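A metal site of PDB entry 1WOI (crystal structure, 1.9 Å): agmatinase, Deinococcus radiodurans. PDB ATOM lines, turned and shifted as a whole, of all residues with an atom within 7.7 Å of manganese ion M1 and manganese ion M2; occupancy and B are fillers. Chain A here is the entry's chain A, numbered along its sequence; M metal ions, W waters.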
ATOM      1  N   ASP A 120      -4.336  29.351   7.871  1.00  0.00           N
ATOM      2  CA  ASP A 120      -5.372  28.531   8.509  1.00  0.00           C
ATOM      3  C   ASP A 120      -5.664  29.155   9.864  1.00  0.00           C
ATOM      4  O   ASP A 120      -4.977  30.073  10.297  1.00  0.00           O
ATOM      5  CB  ASP A 120      -4.942  27.044   8.644  1.00  0.00           C
ATOM      6  CG  ASP A 120      -3.706  26.845   9.507  1.00  0.00           C
ATOM      7  OD1 ASP A 120      -3.695  27.301  10.673  1.00  0.00           O
ATOM      8  OD2 ASP A 120      -2.758  26.183   9.030  1.00  0.00           O
ATOM      9  N   HIS A 121      -6.694  28.674  10.543  1.00  0.00           N
ATOM     10  CA  HIS A 121      -7.069  29.260  11.818  1.00  0.00           C
ATOM     11  C   HIS A 121      -6.043  29.151  12.951  1.00  0.00           C
ATOM     12  O   HIS A 121      -6.170  29.851  13.957  1.00  0.00           O
ATOM     13  CB  HIS A 121      -8.417  28.723  12.286  1.00  0.00           C
ATOM     14  CG  HIS A 121      -9.256  29.752  12.979  1.00  0.00           C
ATOM     15  ND1 HIS A 121     -10.628  29.676  13.031  1.00  0.00           N
ATOM     16  CD2 HIS A 121      -8.913  30.883  13.627  1.00  0.00           C
ATOM     17  CE1 HIS A 121     -11.095  30.729  13.675  1.00  0.00           C
ATOM     18  NE2 HIS A 121     -10.075  31.476  14.050  1.00  0.00           N
ATOM     19  N   SER A 122      -5.039  28.294  12.794  1.00  0.00           N
ATOM     20  CA  SER A 122      -4.041  28.170  13.852  1.00  0.00           C
ATOM     21  C   SER A 122      -3.290  29.488  14.049  1.00  0.00           C
ATOM     22  O   SER A 122      -2.752  29.735  15.121  1.00  0.00           O
ATOM     23  CB  SER A 122      -3.033  27.059  13.537  1.00  0.00           C
ATOM     24  OG  SER A 122      -2.049  27.495  12.625  1.00  0.00           O
ATOM     25  N   SER A 124      -4.378  32.397  14.534  1.00  0.00           N
ATOM     26  CA  SER A 124      -5.020  33.283  15.515  1.00  0.00           C
ATOM     27  C   SER A 124      -4.321  33.220  16.867  1.00  0.00           C
ATOM     28  O   SER A 124      -4.339  34.181  17.624  1.00  0.00           O
ATOM     29  CB  SER A 124      -6.493  32.925  15.682  1.00  0.00           C
ATOM     30  OG  SER A 124      -7.208  33.137  14.476  1.00  0.00           O
ATOM     31  N   GLN A 141     -15.912  35.548  17.548  1.00  0.00           N
ATOM     32  CA  GLN A 141     -15.520  34.581  16.536  1.00  0.00           C
ATOM     33  C   GLN A 141     -16.659  34.120  15.614  1.00  0.00           C
ATOM     34  O   GLN A 141     -17.691  33.644  16.098  1.00  0.00           O
ATOM     35  CB  GLN A 141     -14.930  33.377  17.276  1.00  0.00           C
ATOM     36  CG  GLN A 141     -14.463  32.185  16.455  1.00  0.00           C
ATOM     37  CD  GLN A 141     -14.150  30.992  17.336  1.00  0.00           C
ATOM     38  OE1 GLN A 141     -14.131  31.109  18.568  1.00  0.00           O
ATOM     39  NE2 GLN A 141     -13.890  29.836  16.722  1.00  0.00           N
ATOM     40  N   LEU A 142     -16.468  34.272  14.300  1.00  0.00           N
ATOM     41  CA  LEU A 142     -17.445  33.799  13.327  1.00  0.00           C
ATOM     42  C   LEU A 142     -16.803  32.489  12.872  1.00  0.00           C
ATOM     43  O   LEU A 142     -15.670  32.502  12.373  1.00  0.00           O
ATOM     44  CB  LEU A 142     -17.597  34.758  12.153  1.00  0.00           C
ATOM     45  CG  LEU A 142     -18.233  36.127  12.430  1.00  0.00           C
ATOM     46  CD1 LEU A 142     -18.575  36.801  11.114  1.00  0.00           C
ATOM     47  CD2 LEU A 142     -19.494  35.952  13.249  1.00  0.00           C
ATOM     48  N   ASP A 143     -17.499  31.373  13.028  1.00  0.00           N
ATOM     49  CA  ASP A 143     -16.870  30.094  12.687  1.00  0.00           C
ATOM     50  C   ASP A 143     -17.912  28.983  12.722  1.00  0.00           C
ATOM     51  O   ASP A 143     -18.881  29.062  13.461  1.00  0.00           O
ATOM     52  CB  ASP A 143     -15.803  29.800  13.752  1.00  0.00           C
ATOM     53  CG  ASP A 143     -14.702  28.867  13.278  1.00  0.00           C
ATOM     54  OD1 ASP A 143     -14.987  27.938  12.489  1.00  0.00           O
ATOM     55  OD2 ASP A 143     -13.557  29.079  13.721  1.00  0.00           O
ATOM     56  N   ALA A 144     -17.695  27.950  11.917  1.00  0.00           N
ATOM     57  CA  ALA A 144     -18.582  26.812  11.916  1.00  0.00           C
ATOM     58  C   ALA A 144     -18.065  25.886  13.007  1.00  0.00           C
ATOM     59  O   ALA A 144     -18.784  25.009  13.477  1.00  0.00           O
ATOM     60  CB  ALA A 144     -18.545  26.092  10.558  1.00  0.00           C
ATOM     61  N   HIS A 145     -16.822  26.111  13.423  1.00  0.00           N
ATOM     62  CA  HIS A 145     -16.180  25.283  14.443  1.00  0.00           C
ATOM     63  C   HIS A 145     -15.763  26.073  15.686  1.00  0.00           C
ATOM     64  O   HIS A 145     -15.542  27.286  15.627  1.00  0.00           O
ATOM     65  CB  HIS A 145     -14.953  24.588  13.845  1.00  0.00           C
ATOM     66  CG  HIS A 145     -15.184  24.015  12.477  1.00  0.00           C
ATOM     67  ND1 HIS A 145     -14.802  24.666  11.322  1.00  0.00           N
ATOM     68  CD2 HIS A 145     -15.741  22.848  12.076  1.00  0.00           C
ATOM     69  CE1 HIS A 145     -15.109  23.925  10.276  1.00  0.00           C
ATOM     70  NE2 HIS A 145     -15.681  22.817  10.703  1.00  0.00           N
ATOM     71  N   LEU A 146     -15.659  25.390  16.821  1.00  0.00           N
ATOM     72  CA  LEU A 146     -15.292  26.042  18.078  1.00  0.00           C
ATOM     73  C   LEU A 146     -13.790  26.344  18.197  1.00  0.00           C
ATOM     74  O   LEU A 146     -13.402  27.394  18.713  1.00  0.00           O
ATOM     75  CB  LEU A 146     -15.748  25.176  19.255  1.00  0.00           C
ATOM     76  CG  LEU A 146     -15.620  25.800  20.649  1.00  0.00           C
ATOM     77  CD1 LEU A 146     -16.565  26.995  20.762  1.00  0.00           C
ATOM     78  CD2 LEU A 146     -15.955  24.752  21.704  1.00  0.00           C
ATOM     79  N   ASP A 147     -12.968  25.425  17.713  1.00  0.00           N
ATOM     80  CA  ASP A 147     -11.506  25.558  17.761  1.00  0.00           C
ATOM     81  C   ASP A 147     -10.954  25.835  19.159  1.00  0.00           C
ATOM     82  O   ASP A 147     -10.091  26.701  19.339  1.00  0.00           O
ATOM     83  CB  ASP A 147     -11.028  26.638  16.786  1.00  0.00           C
ATOM     84  CG  ASP A 147     -11.417  26.341  15.344  1.00  0.00           C
ATOM     85  OD1 ASP A 147     -11.527  25.157  14.975  1.00  0.00           O
ATOM     86  OD2 ASP A 147     -11.589  27.307  14.581  1.00  0.00           O
ATOM     87  N   ASN A 159      -5.143  23.694  13.724  1.00  0.00           N
ATOM     88  CA  ASN A 159      -6.097  24.783  13.606  1.00  0.00           C
ATOM     89  C   ASN A 159      -7.343  24.539  14.466  1.00  0.00           C
ATOM     90  O   ASN A 159      -8.280  25.337  14.437  1.00  0.00           O
ATOM     91  CB  ASN A 159      -6.479  25.014  12.132  1.00  0.00           C
ATOM     92  CG  ASN A 159      -7.130  23.800  11.472  1.00  0.00           C
ATOM     93  OD1 ASN A 159      -6.955  22.674  11.938  1.00  0.00           O
ATOM     94  ND2 ASN A 159      -7.894  24.023  10.407  1.00  0.00           N
ATOM     95  N   SER A 160      -7.468  23.521  15.159  1.00  0.00           N
ATOM     96  CA  SER A 160      -8.603  23.231  16.029  1.00  0.00           C
ATOM     97  C   SER A 160      -8.326  23.673  17.470  1.00  0.00           C
ATOM     98  O   SER A 160      -9.190  23.556  18.338  1.00  0.00           O
ATOM     99  CB  SER A 160      -8.917  21.725  16.019  1.00  0.00           C
ATOM    100  OG  SER A 160      -9.266  21.266  14.723  1.00  0.00           O
ATOM    101  N   PRO A 162      -6.319  26.921  18.239  1.00  0.00           N
ATOM    102  CA  PRO A 162      -5.865  28.300  18.469  1.00  0.00           C
ATOM    103  C   PRO A 162      -6.382  29.068  19.681  1.00  0.00           C
ATOM    104  O   PRO A 162      -5.608  29.736  20.365  1.00  0.00           O
ATOM    105  CB  PRO A 162      -6.186  28.994  17.143  1.00  0.00           C
ATOM    106  CG  PRO A 162      -7.386  28.250  16.654  1.00  0.00           C
ATOM    107  CD  PRO A 162      -7.020  26.809  16.945  1.00  0.00           C
ATOM    108  N   PHE A 163      -7.675  28.978  19.955  1.00  0.00           N
ATOM    109  CA  PHE A 163      -8.213  29.717  21.089  1.00  0.00           C
ATOM    110  C   PHE A 163      -7.928  29.055  22.426  1.00  0.00           C
ATOM    111  O   PHE A 163      -7.938  29.728  23.462  1.00  0.00           O
ATOM    112  CB  PHE A 163      -9.709  29.952  20.889  1.00  0.00           C
ATOM    113  CG  PHE A 163      -9.998  30.799  19.692  1.00  0.00           C
ATOM    114  CD1 PHE A 163     -10.585  30.247  18.563  1.00  0.00           C
ATOM    115  CD2 PHE A 163      -9.595  32.127  19.667  1.00  0.00           C
ATOM    116  CE1 PHE A 163     -10.758  31.015  17.414  1.00  0.00           C
ATOM    117  CE2 PHE A 163      -9.756  32.909  18.517  1.00  0.00           C
ATOM    118  CZ  PHE A 163     -10.335  32.342  17.385  1.00  0.00           C
ATOM    119  N   LEU A 181     -21.625  28.112  14.874  1.00  0.00           N
ATOM    120  CA  LEU A 181     -21.354  26.687  15.056  1.00  0.00           C
ATOM    121  C   LEU A 181     -22.435  25.749  14.526  1.00  0.00           C
ATOM    122  O   LEU A 181     -23.627  25.974  14.723  1.00  0.00           O
ATOM    123  CB  LEU A 181     -21.126  26.392  16.551  1.00  0.00           C
ATOM    124  CG  LEU A 181     -19.970  27.144  17.209  1.00  0.00           C
ATOM    125  CD1 LEU A 181     -19.795  26.630  18.640  1.00  0.00           C
ATOM    126  CD2 LEU A 181     -18.685  26.924  16.419  1.00  0.00           C
ATOM    127  N   SER A 227     -12.334  37.562  14.958  1.00  0.00           N
ATOM    128  CA  SER A 227     -11.708  36.446  14.268  1.00  0.00           C
ATOM    129  C   SER A 227     -12.767  35.907  13.322  1.00  0.00           C
ATOM    130  O   SER A 227     -13.749  35.308  13.749  1.00  0.00           O
ATOM    131  CB  SER A 227     -11.277  35.344  15.225  1.00  0.00           C
ATOM    132  OG  SER A 227     -10.665  34.296  14.493  1.00  0.00           O
ATOM    133  N   VAL A 228     -12.565  36.121  12.033  1.00  0.00           N
ATOM    134  CA  VAL A 228     -13.516  35.646  11.040  1.00  0.00           C
ATOM    135  C   VAL A 228     -12.986  34.452  10.270  1.00  0.00           C
ATOM    136  O   VAL A 228     -12.039  34.577   9.493  1.00  0.00           O
ATOM    137  CB  VAL A 228     -13.883  36.759  10.041  1.00  0.00           C
ATOM    138  CG1 VAL A 228     -14.933  36.237   9.036  1.00  0.00           C
ATOM    139  CG2 VAL A 228     -14.416  37.983  10.785  1.00  0.00           C
ATOM    140  N   ASP A 229     -13.599  33.295  10.491  1.00  0.00           N
ATOM    141  CA  ASP A 229     -13.233  32.078   9.777  1.00  0.00           C
ATOM    142  C   ASP A 229     -14.262  32.032   8.647  1.00  0.00           C
ATOM    143  O   ASP A 229     -15.472  31.970   8.912  1.00  0.00           O
ATOM    144  CB  ASP A 229     -13.402  30.860  10.674  1.00  0.00           C
ATOM    145  CG  ASP A 229     -13.017  29.561   9.985  1.00  0.00           C
ATOM    146  OD1 ASP A 229     -13.178  29.436   8.761  1.00  0.00           O
ATOM    147  OD2 ASP A 229     -12.553  28.649  10.696  1.00  0.00           O
ATOM    148  N   VAL A 230     -13.808  32.062   7.403  1.00  0.00           N
ATOM    149  CA  VAL A 230     -14.756  32.056   6.295  1.00  0.00           C
ATOM    150  C   VAL A 230     -15.713  30.876   6.270  1.00  0.00           C
ATOM    151  O   VAL A 230     -16.786  30.973   5.669  1.00  0.00           O
ATOM    152  CB  VAL A 230     -14.038  32.168   4.914  1.00  0.00           C
ATOM    153  CG1 VAL A 230     -13.118  33.382   4.892  1.00  0.00           C
ATOM    154  CG2 VAL A 230     -13.244  30.891   4.617  1.00  0.00           C
ATOM    155  N   ASP A 231     -15.362  29.757   6.924  1.00  0.00           N
ATOM    156  CA  ASP A 231     -16.298  28.633   6.885  1.00  0.00           C
ATOM    157  C   ASP A 231     -17.507  28.868   7.776  1.00  0.00           C
ATOM    158  O   ASP A 231     -18.432  28.045   7.809  1.00  0.00           O
ATOM    159  CB  ASP A 231     -15.623  27.276   7.188  1.00  0.00           C
ATOM    160  CG  ASP A 231     -15.051  27.173   8.587  1.00  0.00           C
ATOM    161  OD1 ASP A 231     -15.644  27.728   9.544  1.00  0.00           O
ATOM    162  OD2 ASP A 231     -13.997  26.515   8.719  1.00  0.00           O
ATOM    163  N   GLY A 232     -17.524  30.010   8.467  1.00  0.00           N
ATOM    164  CA  GLY A 232     -18.694  30.346   9.271  1.00  0.00           C
ATOM    165  C   GLY A 232     -19.820  30.684   8.294  1.00  0.00           C
ATOM    166  O   GLY A 232     -21.001  30.510   8.595  1.00  0.00           O
ATOM    167  N   THR A 241     -13.041  27.020   1.046  1.00  0.00           N
ATOM    168  CA  THR A 241     -12.510  26.796   2.401  1.00  0.00           C
ATOM    169  C   THR A 241     -12.301  25.293   2.561  1.00  0.00           C
ATOM    170  O   THR A 241     -12.974  24.492   1.924  1.00  0.00           O
ATOM    171  CB  THR A 241     -13.487  27.339   3.484  1.00  0.00           C
ATOM    172  OG1 THR A 241     -12.817  27.398   4.752  1.00  0.00           O
ATOM    173  CG2 THR A 241     -14.715  26.454   3.607  1.00  0.00           C
ATOM    174  N   SER A 243     -12.868  22.983   5.119  1.00  0.00           N
ATOM    175  CA  SER A 243     -13.906  22.145   5.705  1.00  0.00           C
ATOM    176  C   SER A 243     -15.277  22.791   5.816  1.00  0.00           C
ATOM    177  O   SER A 243     -15.688  23.200   6.903  1.00  0.00           O
ATOM    178  CB  SER A 243     -13.447  21.705   7.094  1.00  0.00           C
ATOM    179  OG  SER A 243     -12.099  21.257   7.034  1.00  0.00           O
ATOM    180  N   PRO A 244     -15.995  22.884   4.687  1.00  0.00           N
ATOM    181  CA  PRO A 244     -17.334  23.499   4.679  1.00  0.00           C
ATOM    182  C   PRO A 244     -18.390  22.708   5.447  1.00  0.00           C
ATOM    183  O   PRO A 244     -18.330  21.481   5.531  1.00  0.00           O
ATOM    184  CB  PRO A 244     -17.650  23.589   3.187  1.00  0.00           C
ATOM    185  CG  PRO A 244     -16.943  22.395   2.611  1.00  0.00           C
ATOM    186  CD  PRO A 244     -15.605  22.436   3.339  1.00  0.00           C
ATOM    187  N   VAL A 273      -9.403  34.284   8.338  1.00  0.00           N
ATOM    188  CA  VAL A 273      -8.723  33.006   8.131  1.00  0.00           C
ATOM    189  C   VAL A 273      -9.496  31.915   7.384  1.00  0.00           C
ATOM    190  O   VAL A 273     -10.695  32.030   7.174  1.00  0.00           O
ATOM    191  CB  VAL A 273      -8.272  32.419   9.488  1.00  0.00           C
ATOM    192  CG1 VAL A 273      -7.390  33.408  10.211  1.00  0.00           C
ATOM    193  CG2 VAL A 273      -9.501  32.061  10.336  1.00  0.00           C
ATOM    194  N   GLU A 274      -8.754  30.885   6.994  1.00  0.00           N
ATOM    195  CA  GLU A 274      -9.276  29.695   6.301  1.00  0.00           C
ATOM    196  C   GLU A 274      -9.787  29.880   4.866  1.00  0.00           C
ATOM    197  O   GLU A 274     -10.437  28.986   4.319  1.00  0.00           O
ATOM    198  CB  GLU A 274     -10.345  29.015   7.153  1.00  0.00           C
ATOM    199  CG  GLU A 274      -9.852  28.405   8.478  1.00  0.00           C
ATOM    200  CD  GLU A 274      -8.967  27.155   8.308  1.00  0.00           C
ATOM    201  OE1 GLU A 274      -9.023  26.505   7.245  1.00  0.00           O
ATOM    202  OE2 GLU A 274      -8.228  26.814   9.253  1.00  0.00           O
HETATM  203 MN    MN M   1     -13.884  26.750  10.927  1.00  0.00          MN
HETATM  204 MN    MN M   2     -11.924  28.154  12.726  1.00  0.00          MN
HETATM  205  O   HOH W   1     -11.681  25.922  11.935  1.00  0.00           O
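Manganese ion M1 is bound by the side-chain carboxylate (OD2) of Asp 231 (2.2 Å), the side-chain carboxylate (OD1) of Asp 143 (2.3 Å), a ring nitrogen (ND1) of His 145 (2.3 Å), the side-chain carboxylate (OD2) of Asp 229 (2.3 Å), the side-chain carboxylate (OD1) of Asp 231 (2.4 Å) and water W1 (2.6 Å). Manganese ion M1 has six donor atoms within binding distance.
Within 4 Å of manganese ion M1: Asp 143, His 145, Asp 229 and Asp 231.
Four residues have an atom within 4 Å of manganese ion M2: His 121, Asp 143, Asp 147 and Asp 229. Along chain A the residues within 4 Å of manganese ion M2 span positions 121 to 229.
Manganese ion M2 is bound by ND1 of His 121 (2.0 Å), OD2 of Asp 147 (2.1 Å), OD2 of Asp 143 (2.1 Å), OD2 of Asp 229 (2.2 Å) and water W1 (2.4 Å).
The backbone NH (N) of His 121 is in hydrogen-bond range of the side-chain carboxylate (OE2) of Glu 274. A ring nitrogen (NE2) of His 121 sits at hydrogen-bond distance from the side-chain hydroxyl (OG) of Ser 227 (2.9 Å). OG of Ser 124 lies close to NE2 of His 121. O of Asp 147 lies within hydrogen-bond range of N of Phe 163. NE2 of Gln 141 lies close to OD2 of Asp 143 (3.1 Å). The backbone carbonyl oxygen (O) of Leu 142 sits at hydrogen-bond distance from the backbone NH (N) of Asp 229. OD1 of Asp 231 sits close to N of Ala 144, 3.1 Å away. O of His 145 lies within hydrogen-bond range of NE2 of Gln 141.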
